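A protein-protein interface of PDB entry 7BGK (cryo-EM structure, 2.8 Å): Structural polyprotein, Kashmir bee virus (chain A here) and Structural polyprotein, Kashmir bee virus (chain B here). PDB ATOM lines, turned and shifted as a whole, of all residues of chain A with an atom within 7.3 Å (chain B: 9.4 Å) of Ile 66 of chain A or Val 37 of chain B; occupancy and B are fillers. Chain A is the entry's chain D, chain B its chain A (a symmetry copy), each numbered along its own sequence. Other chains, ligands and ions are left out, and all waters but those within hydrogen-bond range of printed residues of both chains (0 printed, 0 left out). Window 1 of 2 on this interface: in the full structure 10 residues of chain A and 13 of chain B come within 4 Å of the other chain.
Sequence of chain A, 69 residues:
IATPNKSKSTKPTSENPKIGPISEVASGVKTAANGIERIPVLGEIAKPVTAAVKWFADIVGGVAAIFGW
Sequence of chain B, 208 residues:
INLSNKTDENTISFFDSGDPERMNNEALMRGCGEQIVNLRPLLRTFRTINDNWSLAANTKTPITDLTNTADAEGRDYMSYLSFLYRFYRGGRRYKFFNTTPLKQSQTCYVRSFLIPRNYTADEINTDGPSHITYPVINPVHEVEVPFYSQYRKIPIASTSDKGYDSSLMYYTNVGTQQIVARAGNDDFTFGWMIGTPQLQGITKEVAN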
ATOM      1  N   TRP A  55     -35.607  -9.534 -21.958  1.00  0.00           N
ATOM      2  CA  TRP A  55     -35.048 -10.450 -22.945  1.00  0.00           C
ATOM      3  C   TRP A  55     -35.498 -10.110 -24.363  1.00  0.00           C
ATOM      4  O   TRP A  55     -34.704 -10.181 -25.312  1.00  0.00           O
ATOM      5  CB  TRP A  55     -35.413 -11.888 -22.584  1.00  0.00           C
ATOM      6  CG  TRP A  55     -36.860 -12.186 -22.541  1.00  0.00           C
ATOM      7  CD1 TRP A  55     -37.677 -12.102 -21.465  1.00  0.00           C
ATOM      8  CD2 TRP A  55     -37.666 -12.641 -23.626  1.00  0.00           C
ATOM      9  NE1 TRP A  55     -38.950 -12.468 -21.809  1.00  0.00           N
ATOM     10  CE2 TRP A  55     -38.969 -12.802 -23.135  1.00  0.00           C
ATOM     11  CE3 TRP A  55     -37.415 -12.920 -24.969  1.00  0.00           C
ATOM     12  CZ2 TRP A  55     -40.010 -13.233 -23.934  1.00  0.00           C
ATOM     13  CZ3 TRP A  55     -38.449 -13.342 -25.755  1.00  0.00           C
ATOM     14  CH2 TRP A  55     -39.731 -13.495 -25.240  1.00  0.00           C
ATOM     15  N   ALA A  57     -36.324  -7.149 -25.434  1.00  0.00           N
ATOM     16  CA  ALA A  57     -35.523  -5.978 -25.756  1.00  0.00           C
ATOM     17  C   ALA A  57     -34.124  -6.369 -26.204  1.00  0.00           C
ATOM     18  O   ALA A  57     -33.585  -5.802 -27.161  1.00  0.00           O
ATOM     19  CB  ALA A  57     -35.453  -5.060 -24.544  1.00  0.00           C
ATOM     20  N   ASP A  58     -33.514  -7.326 -25.509  1.00  0.00           N
ATOM     21  CA  ASP A  58     -32.193  -7.803 -25.890  1.00  0.00           C
ATOM     22  C   ASP A  58     -32.182  -8.408 -27.283  1.00  0.00           C
ATOM     23  O   ASP A  58     -31.191  -8.286 -28.009  1.00  0.00           O
ATOM     24  CB  ASP A  58     -31.723  -8.839 -24.876  1.00  0.00           C
ATOM     25  CG  ASP A  58     -31.555  -8.266 -23.493  1.00  0.00           C
ATOM     26  OD1 ASP A  58     -31.314  -9.048 -22.550  1.00  0.00           O
ATOM     27  OD2 ASP A  58     -31.660  -7.034 -23.347  1.00  0.00           O
ATOM     28  N   ILE A  59     -33.268  -9.071 -27.663  1.00  0.00           N
ATOM     29  CA  ILE A  59     -33.350  -9.671 -28.991  1.00  0.00           C
ATOM     30  C   ILE A  59     -33.567  -8.609 -30.067  1.00  0.00           C
ATOM     31  O   ILE A  59     -32.915  -8.625 -31.117  1.00  0.00           O
ATOM     32  CB  ILE A  59     -34.443 -10.747 -29.002  1.00  0.00           C
ATOM     33  CG1 ILE A  59     -34.002 -11.880 -28.083  1.00  0.00           C
ATOM     34  CG2 ILE A  59     -34.656 -11.281 -30.392  1.00  0.00           C
ATOM     35  CD1 ILE A  59     -34.985 -12.931 -27.886  1.00  0.00           C
ATOM     36  N   VAL A  60     -34.489  -7.675 -29.825  1.00  0.00           N
ATOM     37  CA  VAL A  60     -34.765  -6.624 -30.805  1.00  0.00           C
ATOM     38  C   VAL A  60     -33.572  -5.696 -30.967  1.00  0.00           C
ATOM     39  O   VAL A  60     -33.366  -5.121 -32.042  1.00  0.00           O
ATOM     40  CB  VAL A  60     -36.030  -5.831 -30.431  1.00  0.00           C
ATOM     41  CG1 VAL A  60     -37.235  -6.727 -30.319  1.00  0.00           C
ATOM     42  CG2 VAL A  60     -35.819  -4.960 -29.216  1.00  0.00           C
ATOM     43  N   GLY A  61     -32.769  -5.537 -29.926  1.00  0.00           N
ATOM     44  CA  GLY A  61     -31.536  -4.794 -30.016  1.00  0.00           C
ATOM     45  C   GLY A  61     -30.356  -5.627 -30.423  1.00  0.00           C
ATOM     46  O   GLY A  61     -29.253  -5.098 -30.586  1.00  0.00           O
ATOM     47  N   GLY A  62     -30.558  -6.929 -30.581  1.00  0.00           N
ATOM     48  CA  GLY A  62     -29.496  -7.837 -30.939  1.00  0.00           C
ATOM     49  C   GLY A  62     -28.258  -7.697 -30.091  1.00  0.00           C
ATOM     50  O   GLY A  62     -27.158  -7.598 -30.629  1.00  0.00           O
ATOM     51  N   VAL A  63     -28.409  -7.719 -28.770  1.00  0.00           N
ATOM     52  CA  VAL A  63     -27.250  -7.520 -27.917  1.00  0.00           C
ATOM     53  C   VAL A  63     -26.313  -8.713 -28.053  1.00  0.00           C
ATOM     54  O   VAL A  63     -26.675  -9.780 -28.557  1.00  0.00           O
ATOM     55  CB  VAL A  63     -27.655  -7.291 -26.453  1.00  0.00           C
ATOM     56  CG1 VAL A  63     -28.474  -6.042 -26.324  1.00  0.00           C
ATOM     57  CG2 VAL A  63     -28.418  -8.463 -25.921  1.00  0.00           C
ATOM     58  N   ALA A  64     -25.078  -8.519 -27.609  1.00  0.00           N
ATOM     59  CA  ALA A  64     -24.045  -9.515 -27.829  1.00  0.00           C
ATOM     60  C   ALA A  64     -24.202 -10.729 -26.931  1.00  0.00           C
ATOM     61  O   ALA A  64     -23.599 -11.767 -27.207  1.00  0.00           O
ATOM     62  CB  ALA A  64     -22.674  -8.890 -27.614  1.00  0.00           C
ATOM     63  N   ALA A  65     -24.993 -10.623 -25.866  1.00  0.00           N
ATOM     64  CA  ALA A  65     -25.104 -11.720 -24.919  1.00  0.00           C
ATOM     65  C   ALA A  65     -25.950 -12.848 -25.484  1.00  0.00           C
ATOM     66  O   ALA A  65     -25.676 -14.024 -25.223  1.00  0.00           O
ATOM     67  CB  ALA A  65     -25.693 -11.218 -23.609  1.00  0.00           C
ATOM     68  N   ILE A  66     -26.983 -12.515 -26.259  1.00  0.00           N
ATOM     69  CA  ILE A  66     -27.843 -13.535 -26.837  1.00  0.00           C
ATOM     70  C   ILE A  66     -27.109 -14.381 -27.859  1.00  0.00           C
ATOM     71  O   ILE A  66     -27.652 -15.387 -28.326  1.00  0.00           O
ATOM     72  CB  ILE A  66     -29.096 -12.899 -27.469  1.00  0.00           C
ATOM     73  CG1 ILE A  66     -28.721 -11.900 -28.549  1.00  0.00           C
ATOM     74  CG2 ILE A  66     -29.897 -12.193 -26.429  1.00  0.00           C
ATOM     75  CD1 ILE A  66     -29.788 -11.680 -29.557  1.00  0.00           C
ATOM     76  N   PHE A  67     -25.893 -13.985 -28.225  1.00  0.00           N
ATOM     77  CA  PHE A  67     -25.026 -14.769 -29.084  1.00  0.00           C
ATOM     78  C   PHE A  67     -23.888 -15.428 -28.322  1.00  0.00           C
ATOM     79  O   PHE A  67     -23.048 -16.085 -28.941  1.00  0.00           O
ATOM     80  CB  PHE A  67     -24.447 -13.891 -30.191  1.00  0.00           C
ATOM     81  CG  PHE A  67     -25.477 -13.187 -31.013  1.00  0.00           C
ATOM     82  CD1 PHE A  67     -26.254 -13.879 -31.913  1.00  0.00           C
ATOM     83  CD2 PHE A  67     -25.652 -11.826 -30.902  1.00  0.00           C
ATOM     84  CE1 PHE A  67     -27.189 -13.234 -32.668  1.00  0.00           C
ATOM     85  CE2 PHE A  67     -26.587 -11.180 -31.659  1.00  0.00           C
ATOM     86  CZ  PHE A  67     -27.357 -11.885 -32.545  1.00  0.00           C
ATOM     87  N   GLY A  68     -23.834 -15.267 -27.005  1.00  0.00           N
ATOM     88  CA  GLY A  68     -22.814 -15.885 -26.194  1.00  0.00           C
ATOM     89  C   GLY A  68     -21.590 -15.048 -25.932  1.00  0.00           C
ATOM     90  O   GLY A  68     -20.585 -15.586 -25.457  1.00  0.00           O
ATOM     91  N   TRP A  69     -21.639 -13.756 -26.216  1.00  0.00           N
ATOM     92  CA  TRP A  69     -20.489 -12.892 -26.049  1.00  0.00           C
ATOM     93  C   TRP A  69     -20.696 -11.935 -24.889  1.00  0.00           C
ATOM     94  O   TRP A  69     -20.060 -10.885 -24.822  1.00  0.00           O
ATOM     95  CB  TRP A  69     -20.227 -12.109 -27.327  1.00  0.00           C
ATOM     96  CG  TRP A  69     -20.115 -12.938 -28.561  1.00  0.00           C
ATOM     97  CD1 TRP A  69     -20.866 -12.822 -29.685  1.00  0.00           C
ATOM     98  CD2 TRP A  69     -19.184 -13.994 -28.809  1.00  0.00           C
ATOM     99  NE1 TRP A  69     -20.469 -13.740 -30.618  1.00  0.00           N
ATOM    100  CE2 TRP A  69     -19.436 -14.473 -30.103  1.00  0.00           C
ATOM    101  CE3 TRP A  69     -18.162 -14.582 -28.062  1.00  0.00           C
ATOM    102  CZ2 TRP A  69     -18.709 -15.511 -30.666  1.00  0.00           C
ATOM    103  CZ3 TRP A  69     -17.446 -15.611 -28.623  1.00  0.00           C
ATOM    104  CH2 TRP A  69     -17.720 -16.065 -29.909  1.00  0.00           C
ATOM    105  N   ASN B  25     -43.407 -15.052 -30.850  1.00  0.00           N
ATOM    106  CA  ASN B  25     -43.214 -14.162 -29.715  1.00  0.00           C
ATOM    107  C   ASN B  25     -44.399 -14.216 -28.765  1.00  0.00           C
ATOM    108  O   ASN B  25     -44.228 -14.379 -27.554  1.00  0.00           O
ATOM    109  CB  ASN B  25     -42.985 -12.741 -30.213  1.00  0.00           C
ATOM    110  CG  ASN B  25     -41.696 -12.597 -30.982  1.00  0.00           C
ATOM    111  OD1 ASN B  25     -40.794 -13.424 -30.873  1.00  0.00           O
ATOM    112  ND2 ASN B  25     -41.600 -11.539 -31.764  1.00  0.00           N
ATOM    113  N   LEU B  28     -44.065 -17.314 -26.732  1.00  0.00           N
ATOM    114  CA  LEU B  28     -43.006 -17.316 -25.732  1.00  0.00           C
ATOM    115  C   LEU B  28     -43.335 -16.412 -24.556  1.00  0.00           C
ATOM    116  O   LEU B  28     -42.863 -16.652 -23.440  1.00  0.00           O
ATOM    117  CB  LEU B  28     -41.693 -16.894 -26.367  1.00  0.00           C
ATOM    118  CG  LEU B  28     -41.173 -17.823 -27.452  1.00  0.00           C
ATOM    119  CD1 LEU B  28     -40.128 -17.118 -28.224  1.00  0.00           C
ATOM    120  CD2 LEU B  28     -40.608 -19.084 -26.860  1.00  0.00           C
ATOM    121  N   GLU B  34     -38.630 -16.721 -22.455  1.00  0.00           N
ATOM    122  CA  GLU B  34     -37.299 -16.476 -22.986  1.00  0.00           C
ATOM    123  C   GLU B  34     -37.271 -17.003 -24.411  1.00  0.00           C
ATOM    124  O   GLU B  34     -38.194 -17.688 -24.852  1.00  0.00           O
ATOM    125  CB  GLU B  34     -36.211 -17.122 -22.126  1.00  0.00           C
ATOM    126  CG  GLU B  34     -36.459 -18.562 -21.737  1.00  0.00           C
ATOM    127  CD  GLU B  34     -35.670 -18.993 -20.531  1.00  0.00           C
ATOM    128  OE1 GLU B  34     -35.166 -18.121 -19.802  1.00  0.00           O
ATOM    129  OE2 GLU B  34     -35.556 -20.213 -20.311  1.00  0.00           O
ATOM    130  N   GLN B  35     -36.227 -16.631 -25.144  1.00  0.00           N
ATOM    131  CA  GLN B  35     -36.094 -17.018 -26.545  1.00  0.00           C
ATOM    132  C   GLN B  35     -34.627 -17.330 -26.794  1.00  0.00           C
ATOM    133  O   GLN B  35     -33.791 -16.423 -26.827  1.00  0.00           O
ATOM    134  CB  GLN B  35     -36.617 -15.931 -27.489  1.00  0.00           C
ATOM    135  CG  GLN B  35     -36.104 -15.972 -28.916  1.00  0.00           C
ATOM    136  CD  GLN B  35     -36.913 -16.870 -29.813  1.00  0.00           C
ATOM    137  OE1 GLN B  35     -37.994 -16.501 -30.265  1.00  0.00           O
ATOM    138  NE2 GLN B  35     -36.399 -18.066 -30.075  1.00  0.00           N
ATOM    139  N   ILE B  36     -34.323 -18.612 -26.946  1.00  0.00           N
ATOM    140  CA  ILE B  36     -32.977 -19.065 -27.271  1.00  0.00           C
ATOM    141  C   ILE B  36     -32.784 -18.932 -28.775  1.00  0.00           C
ATOM    142  O   ILE B  36     -33.539 -19.511 -29.562  1.00  0.00           O
ATOM    143  CB  ILE B  36     -32.750 -20.511 -26.807  1.00  0.00           C
ATOM    144  CG1 ILE B  36     -33.279 -20.703 -25.388  1.00  0.00           C
ATOM    145  CG2 ILE B  36     -31.283 -20.865 -26.873  1.00  0.00           C
ATOM    146  CD1 ILE B  36     -33.264 -22.114 -24.910  1.00  0.00           C
ATOM    147  N   VAL B  37     -31.779 -18.158 -29.173  1.00  0.00           N
ATOM    148  CA  VAL B  37     -31.507 -17.898 -30.582  1.00  0.00           C
ATOM    149  C   VAL B  37     -30.153 -18.417 -31.023  1.00  0.00           C
ATOM    150  O   VAL B  37     -29.848 -18.359 -32.223  1.00  0.00           O
ATOM    151  CB  VAL B  37     -31.619 -16.394 -30.910  1.00  0.00           C
ATOM    152  CG1 VAL B  37     -33.019 -15.916 -30.709  1.00  0.00           C
ATOM    153  CG2 VAL B  37     -30.673 -15.578 -30.060  1.00  0.00           C
ATOM    154  N   ASN B  38     -29.335 -18.924 -30.108  1.00  0.00           N
ATOM    155  CA  ASN B  38     -27.985 -19.347 -30.432  1.00  0.00           C
ATOM    156  C   ASN B  38     -27.557 -20.385 -29.412  1.00  0.00           C
ATOM    157  O   ASN B  38     -28.087 -20.446 -28.300  1.00  0.00           O
ATOM    158  CB  ASN B  38     -27.031 -18.149 -30.454  1.00  0.00           C
ATOM    159  CG  ASN B  38     -25.682 -18.481 -31.021  1.00  0.00           C
ATOM    160  OD1 ASN B  38     -25.061 -19.478 -30.662  1.00  0.00           O
ATOM    161  ND2 ASN B  38     -25.218 -17.637 -31.921  1.00  0.00           N
ATOM    162  N   LEU B  39     -26.594 -21.209 -29.810  1.00  0.00           N
ATOM    163  CA  LEU B  39     -26.148 -22.330 -29.001  1.00  0.00           C
ATOM    164  C   LEU B  39     -24.901 -22.044 -28.176  1.00  0.00           C
ATOM    165  O   LEU B  39     -24.526 -22.885 -27.354  1.00  0.00           O
ATOM    166  CB  LEU B  39     -25.894 -23.545 -29.894  1.00  0.00           C
ATOM    167  CG  LEU B  39     -27.070 -23.949 -30.784  1.00  0.00           C
ATOM    168  CD1 LEU B  39     -26.616 -24.829 -31.915  1.00  0.00           C
ATOM    169  CD2 LEU B  39     -28.138 -24.645 -29.991  1.00  0.00           C
ATOM    170  N   ARG B  40     -24.243 -20.905 -28.368  1.00  0.00           N
ATOM    171  CA  ARG B  40     -23.156 -20.515 -27.482  1.00  0.00           C
ATOM    172  C   ARG B  40     -23.652 -20.244 -26.069  1.00  0.00           C
ATOM    173  O   ARG B  40     -22.992 -20.639 -25.097  1.00  0.00           O
ATOM    174  CB  ARG B  40     -22.441 -19.286 -28.022  1.00  0.00           C
ATOM    175  CG  ARG B  40     -21.398 -19.587 -29.029  1.00  0.00           C
ATOM    176  CD  ARG B  40     -20.660 -18.356 -29.462  1.00  0.00           C
ATOM    177  NE  ARG B  40     -20.257 -18.468 -30.858  1.00  0.00           N
ATOM    178  CZ  ARG B  40     -20.967 -18.026 -31.885  1.00  0.00           C
ATOM    179  NH1 ARG B  40     -22.123 -17.420 -31.693  1.00  0.00           N
ATOM    180  NH2 ARG B  40     -20.519 -18.189 -33.114  1.00  0.00           N
ATOM    181  N   PRO B  41     -24.777 -19.553 -25.902  1.00  0.00           N
ATOM    182  CA  PRO B  41     -25.377 -19.473 -24.567  1.00  0.00           C
ATOM    183  C   PRO B  41     -25.435 -20.801 -23.848  1.00  0.00           C
ATOM    184  O   PRO B  41     -25.281 -20.840 -22.623  1.00  0.00           O
ATOM    185  CB  PRO B  41     -26.769 -18.924 -24.874  1.00  0.00           C
ATOM    186  CG  PRO B  41     -26.548 -18.054 -26.011  1.00  0.00           C
ATOM    187  CD  PRO B  41     -25.512 -18.709 -26.858  1.00  0.00           C
ATOM    188  N   LEU B  42     -25.643 -21.898 -24.575  1.00  0.00           N
ATOM    189  CA  LEU B  42     -25.618 -23.218 -23.967  1.00  0.00           C
ATOM    190  C   LEU B  42     -24.207 -23.663 -23.630  1.00  0.00           C
ATOM    191  O   LEU B  42     -24.031 -24.541 -22.782  1.00  0.00           O
ATOM    192  CB  LEU B  42     -26.280 -24.227 -24.895  1.00  0.00           C
ATOM    193  CG  LEU B  42     -27.729 -23.947 -25.284  1.00  0.00           C
ATOM    194  CD1 LEU B  42     -28.235 -25.047 -26.176  1.00  0.00           C
ATOM    195  CD2 LEU B  42     -28.618 -23.787 -24.073  1.00  0.00           C
ATOM    196  N   ARG B  44     -22.260 -21.445 -22.358  1.00  0.00           N
ATOM    197  CA  ARG B  44     -22.037 -20.640 -21.170  1.00  0.00           C
ATOM    198  C   ARG B  44     -22.706 -21.235 -19.940  1.00  0.00           C
ATOM    199  O   ARG B  44     -22.165 -21.121 -18.836  1.00  0.00           O
ATOM    200  CB  ARG B  44     -22.546 -19.220 -21.401  1.00  0.00           C
ATOM    201  CG  ARG B  44     -22.007 -18.558 -22.649  1.00  0.00           C
ATOM    202  CD  ARG B  44     -20.567 -18.173 -22.504  1.00  0.00           C
ATOM    203  NE  ARG B  44     -20.053 -17.568 -23.724  1.00  0.00           N
ATOM    204  CZ  ARG B  44     -19.492 -18.236 -24.723  1.00  0.00           C
ATOM    205  NH1 ARG B  44     -19.363 -19.544 -24.674  1.00  0.00           N
ATOM    206  NH2 ARG B  44     -19.062 -17.587 -25.784  1.00  0.00           N
ATOM    207  N   ASP B 186     -16.337 -16.748 -21.606  1.00  0.00           N
ATOM    208  CA  ASP B 186     -17.055 -15.790 -22.427  1.00  0.00           C
ATOM    209  C   ASP B 186     -16.464 -15.653 -23.830  1.00  0.00           C
ATOM    210  O   ASP B 186     -16.882 -14.766 -24.581  1.00  0.00           O
ATOM    211  CB  ASP B 186     -17.074 -14.434 -21.723  1.00  0.00           C
ATOM    212  CG  ASP B 186     -18.368 -13.669 -21.951  1.00  0.00           C
ATOM    213  OD1 ASP B 186     -19.391 -14.300 -22.289  1.00  0.00           O
ATOM    214  OD2 ASP B 186     -18.361 -12.429 -21.789  1.00  0.00           O
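O of Phe 67 of chain A sits at hydrogen-bond distance from NH1 of Arg 40 of chain B, at 3.2 Å. The backbone carbonyl oxygen (O) of Gly 68 of chain A is in hydrogen-bond range of the guanidinium group (NH2) of Arg 44 of chain B, 2.5 Å away.
Of the 13 printed residues of chain B, 8 touch a printed residue of chain A. Printed residues of chain B that touch a printed residue of chain A: Glu 34, Gln 35, Val 37, Asn 38, Arg 40, Pro 41, Arg 44 and Asp 186. Printed residues of chain A that touch a printed residue of chain B: Trp 55, Ile 59, Ile 66, Phe 67, Gly 68 and Trp 69. Hydrophobic or aromatic side chains of chain A within 4 Å of the printed part of chain B: Trp 55, Ile 59, Phe 67 and Trp 69. Among the printed residues, no Asp or Glu carboxylate lies within 4 Å of a Lys or Arg side-chain nitrogen of the other chain.
Of chain B, only Gln 35 (3.4 Å) comes within 4 Å of Ile 59 of chain A. No residue of chain B comes within 4 Å of Gly 62 of chain A. Printed residues of chain B within 4 Å of Ile 66 of chain A: Val 37, Asn 38 and Pro 41. Of the printed residues of chain B, Gly 68 of chain A touches Arg 40, Pro 41, Arg 44 and Asp 186. Of chain A, only Ile 66 comes within 4 Å of Val 37 of chain B. Printed residues of chain A within 4 Å of Asn 38 of chain B: Ile 66 and Phe 67. Of the printed residues of chain A, Arg 40 of chain B touches Phe 67, Gly 68 and Trp 69. Of the printed residues of chain A, Arg 44 of chain B touches Gly 68 and Trp 69. The nearest residue of chain B that does not touch Ile 66 of chain A is Gln 35 of chain B (5.8 Å). The nearest residue of chain A that does not touch Val 37 of chain B is Ile 59 of chain A (4.6 Å).
Among the printed residues, merely in contact across the chains: Trp 69 of chain A with Arg 40 of chain B (3.3 Å), Ile 59 of chain A with Gln 35 of chain B (3.4 Å), Ile 66 of chain A with Val 37 of chain B (3.5 Å), Ile 66 of chain A with Asn 38 of chain B (3.5 Å), Trp 55 of chain A with Gln 35 of chain B (3.6 Å), Gly 68 of chain A with Asp 186 of chain B (3.6 Å), Ile 66 of chain A with Pro 41 of chain B (3.7 Å), Trp 69 of chain A with Asp 186 of chain B (3.7 Å), Trp 69 of chain A with Arg 44 of chain B (3.8 Å), Gly 68 of chain A with Pro 41 of chain B (3.8 Å), Gly 68 of chain A with Arg 40 of chain B (3.9 Å), Phe 67 of chain A with Asn 38 of chain B (3.9 Å), Trp 55 of chain A with Glu 34 of chain B (3.9 Å) and Phe 67 of chain A with Pro 41 of chain B (3.9 Å).
O of Ala 64 of chain A lies within hydrogen-bond range of N of Trp 69 of chain A (3.0 Å). The backbone NH (N) of Arg 40 of chain B lies within hydrogen-bond range of the side-chain amide oxygen (OD1) of Asn 38 of chain B (2.8 Å). OD1 of Asp 186 of chain B lies within salt-bridge range of NE of Arg 44 of chain B (3.6 Å).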
